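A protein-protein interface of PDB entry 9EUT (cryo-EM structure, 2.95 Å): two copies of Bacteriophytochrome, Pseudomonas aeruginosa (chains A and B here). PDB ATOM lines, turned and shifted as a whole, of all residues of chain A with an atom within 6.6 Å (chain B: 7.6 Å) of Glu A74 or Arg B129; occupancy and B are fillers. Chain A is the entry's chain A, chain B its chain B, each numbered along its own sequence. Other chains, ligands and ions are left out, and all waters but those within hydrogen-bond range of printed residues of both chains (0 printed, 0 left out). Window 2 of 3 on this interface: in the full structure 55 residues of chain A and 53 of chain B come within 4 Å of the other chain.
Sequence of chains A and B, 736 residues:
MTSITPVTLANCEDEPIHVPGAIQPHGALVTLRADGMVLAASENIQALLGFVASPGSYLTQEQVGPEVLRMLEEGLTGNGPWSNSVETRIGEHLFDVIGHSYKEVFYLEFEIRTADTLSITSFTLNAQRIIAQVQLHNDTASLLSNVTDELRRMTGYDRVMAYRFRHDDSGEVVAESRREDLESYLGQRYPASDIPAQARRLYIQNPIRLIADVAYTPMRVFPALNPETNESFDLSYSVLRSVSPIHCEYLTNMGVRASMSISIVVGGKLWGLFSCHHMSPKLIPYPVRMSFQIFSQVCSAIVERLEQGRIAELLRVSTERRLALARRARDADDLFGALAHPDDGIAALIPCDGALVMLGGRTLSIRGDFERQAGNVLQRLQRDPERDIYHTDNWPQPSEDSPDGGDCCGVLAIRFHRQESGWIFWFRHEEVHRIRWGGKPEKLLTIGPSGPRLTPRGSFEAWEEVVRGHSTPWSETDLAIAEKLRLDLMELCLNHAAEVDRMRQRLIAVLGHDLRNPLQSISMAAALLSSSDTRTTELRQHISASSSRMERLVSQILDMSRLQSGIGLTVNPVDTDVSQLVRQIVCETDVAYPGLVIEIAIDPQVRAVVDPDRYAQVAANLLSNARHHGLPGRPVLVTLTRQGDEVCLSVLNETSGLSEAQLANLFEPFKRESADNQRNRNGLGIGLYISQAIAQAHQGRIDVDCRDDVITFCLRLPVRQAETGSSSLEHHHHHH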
ATOM      1  N   LEU A  69       5.457 -20.760 -23.803  1.00  0.00           N
ATOM      2  CA  LEU A  69       4.863 -22.014 -24.251  1.00  0.00           C
ATOM      3  C   LEU A  69       5.909 -22.964 -24.822  1.00  0.00           C
ATOM      4  O   LEU A  69       5.821 -24.173 -24.602  1.00  0.00           O
ATOM      5  CB  LEU A  69       3.756 -21.754 -25.264  1.00  0.00           C
ATOM      6  CG  LEU A  69       2.511 -21.182 -24.603  1.00  0.00           C
ATOM      7  CD1 LEU A  69       1.458 -20.862 -25.628  1.00  0.00           C
ATOM      8  CD2 LEU A  69       1.987 -22.197 -23.615  1.00  0.00           C
ATOM      9  N   ARG A  70       6.895 -22.458 -25.563  1.00  0.00           N
ATOM     10  CA  ARG A  70       7.961 -23.339 -26.034  1.00  0.00           C
ATOM     11  C   ARG A  70       8.700 -23.971 -24.864  1.00  0.00           C
ATOM     12  O   ARG A  70       8.944 -25.187 -24.850  1.00  0.00           O
ATOM     13  CB  ARG A  70       8.953 -22.567 -26.904  1.00  0.00           C
ATOM     14  CG  ARG A  70       8.510 -22.278 -28.320  1.00  0.00           C
ATOM     15  CD  ARG A  70       9.527 -21.369 -28.997  1.00  0.00           C
ATOM     16  NE  ARG A  70       9.011 -20.772 -30.221  1.00  0.00           N
ATOM     17  CZ  ARG A  70       9.163 -19.496 -30.549  1.00  0.00           C
ATOM     18  NH1 ARG A  70       9.922 -18.684 -29.832  1.00  0.00           N
ATOM     19  NH2 ARG A  70       8.559 -19.029 -31.638  1.00  0.00           N
ATOM     20  N   MET A  71       9.012 -23.166 -23.842  1.00  0.00           N
ATOM     21  CA  MET A  71       9.711 -23.682 -22.669  1.00  0.00           C
ATOM     22  C   MET A  71       8.872 -24.721 -21.942  1.00  0.00           C
ATOM     23  O   MET A  71       9.358 -25.807 -21.602  1.00  0.00           O
ATOM     24  CB  MET A  71      10.071 -22.532 -21.732  1.00  0.00           C
ATOM     25  CG  MET A  71      10.541 -22.974 -20.359  1.00  0.00           C
ATOM     26  SD  MET A  71      10.961 -21.572 -19.318  1.00  0.00           S
ATOM     27  CE  MET A  71       9.338 -20.883 -19.066  1.00  0.00           C
ATOM     28  N   LEU A  72       7.602 -24.410 -21.706  1.00  0.00           N
ATOM     29  CA  LEU A  72       6.737 -25.333 -20.990  1.00  0.00           C
ATOM     30  C   LEU A  72       6.559 -26.625 -21.770  1.00  0.00           C
ATOM     31  O   LEU A  72       6.589 -27.711 -21.188  1.00  0.00           O
ATOM     32  CB  LEU A  72       5.393 -24.669 -20.716  1.00  0.00           C
ATOM     33  CG  LEU A  72       4.382 -25.543 -19.995  1.00  0.00           C
ATOM     34  CD1 LEU A  72       4.898 -25.856 -18.612  1.00  0.00           C
ATOM     35  CD2 LEU A  72       3.045 -24.839 -19.938  1.00  0.00           C
ATOM     36  N   GLU A  73       6.305 -26.530 -23.078  1.00  0.00           N
ATOM     37  CA  GLU A  73       6.150 -27.730 -23.893  1.00  0.00           C
ATOM     38  C   GLU A  73       7.391 -28.610 -23.820  1.00  0.00           C
ATOM     39  O   GLU A  73       7.282 -29.832 -23.682  1.00  0.00           O
ATOM     40  CB  GLU A  73       5.844 -27.353 -25.341  1.00  0.00           C
ATOM     41  CG  GLU A  73       4.438 -26.824 -25.572  1.00  0.00           C
ATOM     42  CD  GLU A  73       4.239 -26.308 -26.987  1.00  0.00           C
ATOM     43  OE1 GLU A  73       5.144 -26.499 -27.825  1.00  0.00           O
ATOM     44  OE2 GLU A  73       3.178 -25.711 -27.265  1.00  0.00           O
ATOM     45  N   GLU A  74       8.583 -28.008 -23.907  1.00  0.00           N
ATOM     46  CA  GLU A  74       9.804 -28.798 -23.769  1.00  0.00           C
ATOM     47  C   GLU A  74       9.947 -29.388 -22.373  1.00  0.00           C
ATOM     48  O   GLU A  74      10.619 -30.410 -22.198  1.00  0.00           O
ATOM     49  CB  GLU A  74      11.031 -27.951 -24.096  1.00  0.00           C
ATOM     50  CG  GLU A  74      11.251 -27.710 -25.574  1.00  0.00           C
ATOM     51  CD  GLU A  74      12.722 -27.660 -25.934  1.00  0.00           C
ATOM     52  OE1 GLU A  74      13.418 -28.679 -25.737  1.00  0.00           O
ATOM     53  OE2 GLU A  74      13.184 -26.602 -26.407  1.00  0.00           O
ATOM     54  N   GLY A  75       9.337 -28.757 -21.376  1.00  0.00           N
ATOM     55  CA  GLY A  75       9.370 -29.238 -20.008  1.00  0.00           C
ATOM     56  C   GLY A  75       8.447 -30.398 -19.699  1.00  0.00           C
ATOM     57  O   GLY A  75       8.872 -31.418 -19.155  1.00  0.00           O
ATOM     58  N   LEU A  76       7.172 -30.231 -20.040  1.00  0.00           N
ATOM     59  CA  LEU A  76       6.166 -31.258 -19.787  1.00  0.00           C
ATOM     60  C   LEU A  76       6.471 -32.549 -20.536  1.00  0.00           C
ATOM     61  O   LEU A  76       6.300 -33.645 -19.987  1.00  0.00           O
ATOM     62  CB  LEU A  76       4.790 -30.742 -20.205  1.00  0.00           C
ATOM     63  CG  LEU A  76       4.160 -29.539 -19.512  1.00  0.00           C
ATOM     64  CD1 LEU A  76       2.890 -29.171 -20.230  1.00  0.00           C
ATOM     65  CD2 LEU A  76       3.875 -29.827 -18.066  1.00  0.00           C
ATOM     66  N   THR A  77       6.922 -32.448 -21.781  1.00  0.00           N
ATOM     67  CA  THR A  77       7.196 -33.631 -22.587  1.00  0.00           C
ATOM     68  C   THR A  77       8.606 -34.180 -22.412  1.00  0.00           C
ATOM     69  O   THR A  77       8.884 -35.282 -22.893  1.00  0.00           O
ATOM     70  CB  THR A  77       6.953 -33.330 -24.067  1.00  0.00           C
ATOM     71  OG1 THR A  77       7.924 -32.385 -24.530  1.00  0.00           O
ATOM     72  CG2 THR A  77       5.564 -32.751 -24.261  1.00  0.00           C
ATOM     73  N   GLY A  78       9.494 -33.457 -21.744  1.00  0.00           N
ATOM     74  CA  GLY A  78      10.840 -33.939 -21.527  1.00  0.00           C
ATOM     75  C   GLY A  78      10.877 -35.080 -20.523  1.00  0.00           C
ATOM     76  O   GLY A  78       9.876 -35.470 -19.922  1.00  0.00           O
ATOM     77  N   ASN A  79      12.076 -35.626 -20.345  1.00  0.00           N
ATOM     78  CA  ASN A  79      12.317 -36.728 -19.427  1.00  0.00           C
ATOM     79  C   ASN A  79      13.343 -36.333 -18.375  1.00  0.00           C
ATOM     80  O   ASN A  79      14.255 -35.543 -18.634  1.00  0.00           O
ATOM     81  CB  ASN A  79      12.791 -37.981 -20.171  1.00  0.00           C
ATOM     82  CG  ASN A  79      11.689 -38.625 -20.988  1.00  0.00           C
ATOM     83  OD1 ASN A  79      10.714 -39.137 -20.437  1.00  0.00           O
ATOM     84  ND2 ASN A  79      11.840 -38.611 -22.307  1.00  0.00           N
ATOM     85  N   TRP A  82      13.464 -31.304 -14.639  1.00  0.00           N
ATOM     86  CA  TRP A  82      13.302 -30.160 -15.520  1.00  0.00           C
ATOM     87  C   TRP A  82      13.572 -28.868 -14.773  1.00  0.00           C
ATOM     88  O   TRP A  82      13.118 -28.681 -13.644  1.00  0.00           O
ATOM     89  CB  TRP A  82      11.911 -30.112 -16.152  1.00  0.00           C
ATOM     90  CG  TRP A  82      11.738 -28.930 -17.051  1.00  0.00           C
ATOM     91  CD1 TRP A  82      12.466 -28.640 -18.166  1.00  0.00           C
ATOM     92  CD2 TRP A  82      10.736 -27.913 -16.953  1.00  0.00           C
ATOM     93  NE1 TRP A  82      12.009 -27.483 -18.741  1.00  0.00           N
ATOM     94  CE2 TRP A  82      10.941 -27.022 -18.017  1.00  0.00           C
ATOM     95  CE3 TRP A  82       9.696 -27.663 -16.062  1.00  0.00           C
ATOM     96  CZ2 TRP A  82      10.146 -25.906 -18.213  1.00  0.00           C
ATOM     97  CZ3 TRP A  82       8.910 -26.558 -16.260  1.00  0.00           C
ATOM     98  CH2 TRP A  82       9.137 -25.691 -17.325  1.00  0.00           C
ATOM     99  N   SER A  83      14.329 -27.989 -15.416  1.00  0.00           N
ATOM    100  CA  SER A  83      14.602 -26.658 -14.889  1.00  0.00           C
ATOM    101  C   SER A  83      15.049 -25.805 -16.059  1.00  0.00           C
ATOM    102  O   SER A  83      16.070 -26.103 -16.682  1.00  0.00           O
ATOM    103  CB  SER A  83      15.673 -26.701 -13.807  1.00  0.00           C
ATOM    104  OG  SER A  83      15.902 -25.411 -13.267  1.00  0.00           O
ATOM    105  N   ASN A  84      14.293 -24.756 -16.361  1.00  0.00           N
ATOM    106  CA  ASN A  84      14.630 -23.881 -17.470  1.00  0.00           C
ATOM    107  C   ASN A  84      14.081 -22.496 -17.169  1.00  0.00           C
ATOM    108  O   ASN A  84      13.215 -22.327 -16.312  1.00  0.00           O
ATOM    109  CB  ASN A  84      14.076 -24.428 -18.791  1.00  0.00           C
ATOM    110  CG  ASN A  84      14.637 -23.715 -20.002  1.00  0.00           C
ATOM    111  OD1 ASN A  84      15.684 -23.078 -19.930  1.00  0.00           O
ATOM    112  ND2 ASN A  84      13.937 -23.816 -21.123  1.00  0.00           N
ATOM    113  N   SER A  85      14.587 -21.505 -17.898  1.00  0.00           N
ATOM    114  CA  SER A  85      14.121 -20.136 -17.760  1.00  0.00           C
ATOM    115  C   SER A  85      14.215 -19.443 -19.107  1.00  0.00           C
ATOM    116  O   SER A  85      15.011 -19.824 -19.966  1.00  0.00           O
ATOM    117  CB  SER A  85      14.937 -19.370 -16.720  1.00  0.00           C
ATOM    118  OG  SER A  85      16.285 -19.261 -17.132  1.00  0.00           O
ATOM    119  N   MET A 290      21.701 -17.518 -10.768  1.00  0.00           N
ATOM    120  CA  MET A 290      22.107 -18.772 -11.397  1.00  0.00           C
ATOM    121  C   MET A 290      23.623 -18.935 -11.366  1.00  0.00           C
ATOM    122  O   MET A 290      24.143 -20.031 -11.105  1.00  0.00           O
ATOM    123  CB  MET A 290      21.589 -18.822 -12.829  1.00  0.00           C
ATOM    124  CG  MET A 290      20.515 -19.858 -13.060  1.00  0.00           C
ATOM    125  SD  MET A 290      21.183 -21.520 -13.209  1.00  0.00           S
ATOM    126  CE  MET A 290      21.833 -21.453 -14.874  1.00  0.00           C
ATOM    127  N   PHE B 123      23.254 -21.609 -28.516  1.00  0.00           N
ATOM    128  CA  PHE B 123      23.765 -22.765 -27.786  1.00  0.00           C
ATOM    129  C   PHE B 123      23.973 -22.440 -26.316  1.00  0.00           C
ATOM    130  O   PHE B 123      23.976 -23.341 -25.472  1.00  0.00           O
ATOM    131  CB  PHE B 123      25.099 -23.223 -28.380  1.00  0.00           C
ATOM    132  CG  PHE B 123      24.993 -23.877 -29.726  1.00  0.00           C
ATOM    133  CD1 PHE B 123      23.789 -23.938 -30.405  1.00  0.00           C
ATOM    134  CD2 PHE B 123      26.115 -24.431 -30.317  1.00  0.00           C
ATOM    135  CE1 PHE B 123      23.707 -24.540 -31.644  1.00  0.00           C
ATOM    136  CE2 PHE B 123      26.041 -25.032 -31.552  1.00  0.00           C
ATOM    137  CZ  PHE B 123      24.834 -25.089 -32.218  1.00  0.00           C
ATOM    138  N   THR B 124      24.174 -21.160 -25.998  1.00  0.00           N
ATOM    139  CA  THR B 124      24.303 -20.734 -24.610  1.00  0.00           C
ATOM    140  C   THR B 124      23.041 -21.025 -23.802  1.00  0.00           C
ATOM    141  O   THR B 124      23.116 -21.172 -22.578  1.00  0.00           O
ATOM    142  CB  THR B 124      24.660 -19.247 -24.550  1.00  0.00           C
ATOM    143  OG1 THR B 124      25.163 -18.927 -23.248  1.00  0.00           O
ATOM    144  CG2 THR B 124      23.448 -18.380 -24.853  1.00  0.00           C
ATOM    145  N   LEU B 125      21.877 -21.098 -24.452  1.00  0.00           N
ATOM    146  CA  LEU B 125      20.656 -21.446 -23.733  1.00  0.00           C
ATOM    147  C   LEU B 125      20.609 -22.934 -23.405  1.00  0.00           C
ATOM    148  O   LEU B 125      20.207 -23.321 -22.299  1.00  0.00           O
ATOM    149  CB  LEU B 125      19.437 -21.046 -24.559  1.00  0.00           C
ATOM    150  CG  LEU B 125      19.320 -19.564 -24.914  1.00  0.00           C
ATOM    151  CD1 LEU B 125      18.111 -19.326 -25.796  1.00  0.00           C
ATOM    152  CD2 LEU B 125      19.247 -18.714 -23.665  1.00  0.00           C
ATOM    153  N   ASN B 126      21.041 -23.781 -24.340  1.00  0.00           N
ATOM    154  CA  ASN B 126      21.130 -25.206 -24.052  1.00  0.00           C
ATOM    155  C   ASN B 126      22.162 -25.456 -22.965  1.00  0.00           C
ATOM    156  O   ASN B 126      22.002 -26.357 -22.129  1.00  0.00           O
ATOM    157  CB  ASN B 126      21.472 -25.982 -25.319  1.00  0.00           C
ATOM    158  CG  ASN B 126      20.351 -25.965 -26.331  1.00  0.00           C
ATOM    159  OD1 ASN B 126      20.298 -25.099 -27.202  1.00  0.00           O
ATOM    160  ND2 ASN B 126      19.446 -26.929 -26.225  1.00  0.00           N
ATOM    161  N   ALA B 127      23.242 -24.676 -22.977  1.00  0.00           N
ATOM    162  CA  ALA B 127      24.235 -24.772 -21.919  1.00  0.00           C
ATOM    163  C   ALA B 127      23.616 -24.423 -20.578  1.00  0.00           C
ATOM    164  O   ALA B 127      23.872 -25.095 -19.575  1.00  0.00           O
ATOM    165  CB  ALA B 127      25.413 -23.853 -22.219  1.00  0.00           C
ATOM    166  N   GLN B 128      22.821 -23.352 -20.536  1.00  0.00           N
ATOM    167  CA  GLN B 128      22.131 -22.982 -19.307  1.00  0.00           C
ATOM    168  C   GLN B 128      21.251 -24.112 -18.799  1.00  0.00           C
ATOM    169  O   GLN B 128      21.268 -24.433 -17.605  1.00  0.00           O
ATOM    170  CB  GLN B 128      21.272 -21.741 -19.544  1.00  0.00           C
ATOM    171  CG  GLN B 128      22.032 -20.444 -19.630  1.00  0.00           C
ATOM    172  CD  GLN B 128      21.225 -19.344 -20.288  1.00  0.00           C
ATOM    173  OE1 GLN B 128      21.780 -18.445 -20.921  1.00  0.00           O
ATOM    174  NE2 GLN B 128      19.905 -19.415 -20.151  1.00  0.00           N
ATOM    175  N   ARG B 129      20.486 -24.742 -19.693  1.00  0.00           N
ATOM    176  CA  ARG B 129      19.645 -25.862 -19.277  1.00  0.00           C
ATOM    177  C   ARG B 129      20.464 -27.016 -18.714  1.00  0.00           C
ATOM    178  O   ARG B 129      20.198 -27.487 -17.604  1.00  0.00           O
ATOM    179  CB  ARG B 129      18.753 -26.351 -20.415  1.00  0.00           C
ATOM    180  CG  ARG B 129      17.629 -25.402 -20.721  1.00  0.00           C
ATOM    181  CD  ARG B 129      16.941 -25.727 -22.025  1.00  0.00           C
ATOM    182  NE  ARG B 129      16.191 -26.972 -21.896  1.00  0.00           N
ATOM    183  CZ  ARG B 129      15.385 -27.463 -22.825  1.00  0.00           C
ATOM    184  NH1 ARG B 129      15.215 -26.855 -23.987  1.00  0.00           N
ATOM    185  NH2 ARG B 129      14.723 -28.591 -22.578  1.00  0.00           N
ATOM    186  N   ILE B 130      21.466 -27.485 -19.459  1.00  0.00           N
ATOM    187  CA  ILE B 130      22.279 -28.602 -18.979  1.00  0.00           C
ATOM    188  C   ILE B 130      22.925 -28.277 -17.637  1.00  0.00           C
ATOM    189  O   ILE B 130      22.870 -29.078 -16.700  1.00  0.00           O
ATOM    190  CB  ILE B 130      23.337 -28.994 -20.024  1.00  0.00           C
ATOM    191  CG1 ILE B 130      22.676 -29.493 -21.304  1.00  0.00           C
ATOM    192  CG2 ILE B 130      24.245 -30.072 -19.477  1.00  0.00           C
ATOM    193  CD1 ILE B 130      23.663 -30.047 -22.299  1.00  0.00           C
ATOM    194  N   ILE B 131      23.552 -27.105 -17.520  1.00  0.00           N
ATOM    195  CA  ILE B 131      24.211 -26.740 -16.267  1.00  0.00           C
ATOM    196  C   ILE B 131      23.209 -26.691 -15.119  1.00  0.00           C
ATOM    197  O   ILE B 131      23.501 -27.130 -14.001  1.00  0.00           O
ATOM    198  CB  ILE B 131      24.961 -25.406 -16.419  1.00  0.00           C
ATOM    199  CG1 ILE B 131      26.122 -25.551 -17.397  1.00  0.00           C
ATOM    200  CG2 ILE B 131      25.503 -24.964 -15.092  1.00  0.00           C
ATOM    201  CD1 ILE B 131      26.652 -24.232 -17.904  1.00  0.00           C
ATOM    202  N   ALA B 132      22.008 -26.180 -15.378  1.00  0.00           N
ATOM    203  CA  ALA B 132      20.988 -26.092 -14.338  1.00  0.00           C
ATOM    204  C   ALA B 132      20.343 -27.441 -14.042  1.00  0.00           C
ATOM    205  O   ALA B 132      20.102 -27.775 -12.878  1.00  0.00           O
ATOM    206  CB  ALA B 132      19.918 -25.079 -14.740  1.00  0.00           C
ATOM    207  N   GLN B 133      20.048 -28.213 -15.083  1.00  0.00           N
ATOM    208  CA  GLN B 133      19.357 -29.488 -14.927  1.00  0.00           C
ATOM    209  C   GLN B 133      20.223 -30.559 -14.271  1.00  0.00           C
ATOM    210  O   GLN B 133      19.698 -31.408 -13.546  1.00  0.00           O
ATOM    211  CB  GLN B 133      18.908 -29.959 -16.305  1.00  0.00           C
ATOM    212  CG  GLN B 133      17.770 -30.915 -16.340  1.00  0.00           C
ATOM    213  CD  GLN B 133      16.842 -30.588 -17.478  1.00  0.00           C
ATOM    214  OE1 GLN B 133      15.992 -29.711 -17.370  1.00  0.00           O
ATOM    215  NE2 GLN B 133      17.007 -31.285 -18.589  1.00  0.00           N
ATOM    216  N   VAL B 134      21.534 -30.554 -14.525  1.00  0.00           N
ATOM    217  CA  VAL B 134      22.444 -31.543 -13.938  1.00  0.00           C
ATOM    218  C   VAL B 134      22.388 -31.558 -12.415  1.00  0.00           C
ATOM    219  O   VAL B 134      22.516 -32.619 -11.792  1.00  0.00           O
ATOM    220  CB  VAL B 134      23.878 -31.276 -14.439  1.00  0.00           C
ATOM    221  CG1 VAL B 134      24.906 -31.908 -13.527  1.00  0.00           C
ATOM    222  CG2 VAL B 134      24.049 -31.806 -15.833  1.00  0.00           C
ATOM    223  N   GLN B 135      22.146 -30.408 -11.794  1.00  0.00           N
ATOM    224  CA  GLN B 135      22.124 -30.300 -10.340  1.00  0.00           C
ATOM    225  C   GLN B 135      20.973 -31.048  -9.681  1.00  0.00           C
ATOM    226  O   GLN B 135      20.999 -31.217  -8.458  1.00  0.00           O
ATOM    227  CB  GLN B 135      22.091 -28.826  -9.944  1.00  0.00           C
ATOM    228  CG  GLN B 135      23.137 -27.991 -10.668  1.00  0.00           C
ATOM    229  CD  GLN B 135      23.071 -26.520 -10.318  1.00  0.00           C
ATOM    230  OE1 GLN B 135      22.655 -26.151  -9.222  1.00  0.00           O
ATOM    231  NE2 GLN B 135      23.484 -25.672 -11.249  1.00  0.00           N
ATOM    232  N   GLU B 150      21.263 -34.887 -23.530  1.00  0.00           N
ATOM    233  CA  GLU B 150      21.241 -33.434 -23.632  1.00  0.00           C
ATOM    234  C   GLU B 150      22.446 -32.919 -24.405  1.00  0.00           C
ATOM    235  O   GLU B 150      22.315 -32.012 -25.228  1.00  0.00           O
ATOM    236  CB  GLU B 150      21.180 -32.810 -22.242  1.00  0.00           C
ATOM    237  CG  GLU B 150      19.956 -33.213 -21.447  1.00  0.00           C
ATOM    238  CD  GLU B 150      19.367 -32.059 -20.670  1.00  0.00           C
ATOM    239  OE1 GLU B 150      18.923 -31.084 -21.310  1.00  0.00           O
ATOM    240  OE2 GLU B 150      19.344 -32.125 -19.423  1.00  0.00           O
ATOM    241  N   ARG B 153      21.848 -33.527 -28.116  1.00  0.00           N
ATOM    242  CA  ARG B 153      20.865 -32.611 -28.692  1.00  0.00           C
ATOM    243  C   ARG B 153      21.427 -31.203 -28.814  1.00  0.00           C
ATOM    244  O   ARG B 153      21.225 -30.530 -29.830  1.00  0.00           O
ATOM    245  CB  ARG B 153      19.599 -32.596 -27.841  1.00  0.00           C
ATOM    246  CG  ARG B 153      18.795 -33.874 -27.908  1.00  0.00           C
ATOM    247  CD  ARG B 153      17.659 -33.860 -26.905  1.00  0.00           C
ATOM    248  NE  ARG B 153      17.034 -35.171 -26.791  1.00  0.00           N
ATOM    249  CZ  ARG B 153      16.663 -35.722 -25.644  1.00  0.00           C
ATOM    250  NH1 ARG B 153      16.770 -35.069 -24.498  1.00  0.00           N
ATOM    251  NH2 ARG B 153      16.157 -36.951 -25.649  1.00  0.00           N
ATOM    252  N   MET B 154      22.137 -30.745 -27.786  1.00  0.00           N
ATOM    253  CA  MET B 154      22.728 -29.413 -27.783  1.00  0.00           C
ATOM    254  C   MET B 154      23.793 -29.259 -28.859  1.00  0.00           C
ATOM    255  O   MET B 154      23.691 -28.397 -29.736  1.00  0.00           O
ATOM    256  CB  MET B 154      23.331 -29.136 -26.409  1.00  0.00           C
ATOM    257  CG  MET B 154      24.234 -27.938 -26.373  1.00  0.00           C
ATOM    258  SD  MET B 154      24.897 -27.639 -24.736  1.00  0.00           S
ATOM    259  CE  MET B 154      25.887 -26.190 -25.065  1.00  0.00           C
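Among the printed residues, merely in contact across the chains: Trp A82 with Gln B133 (3.3 Å) and Asn A84 with Arg B129 (3.1 Å).
Glu A74 touches one residue of chain B.
Of the printed residues of chain B, Trp A82 touches Gln B133 (3.3 Å).
Of the printed residues of chain B, Ser A83 touches Gln B133.
Printed residues of chain B within 4 Å of Asn A84: Arg B129 (3.1 Å).
Of chain A, only Glu A74 and Asn A84 come within 4 Å of Arg B129.
Of the printed residues of chain A, Gln B133 touches Trp A82 and Ser A83.
The nearest printed residue of chain A that does not touch Gln B133 is Asn A79 (5.1 Å).
No position is printed for both chains.
Of the 4 pairs that touch across the chains among the printed residues, none has its exchanged pair printed and touching as well.
The side-chain amide nitrogen of Gln B133 sits at hydrogen-bond distance from the side-chain carboxylate of Glu B150.
Of the 16 printed residues of chain B, 2 touch a printed residue of chain A.
Along chain B the printed residues that touch a printed residue of chain A span positions 129 to 133.
The backbone NH (N) of Ser A83 lies within hydrogen-bond range of the side-chain amide oxygen (OE1) of Gln B133, 3.1 Å away.
The side-chain carboxylate (OE1) of Glu A74 is in salt-bridge range of the guanidinium group (NH1) of Arg B129 (3.1 Å).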
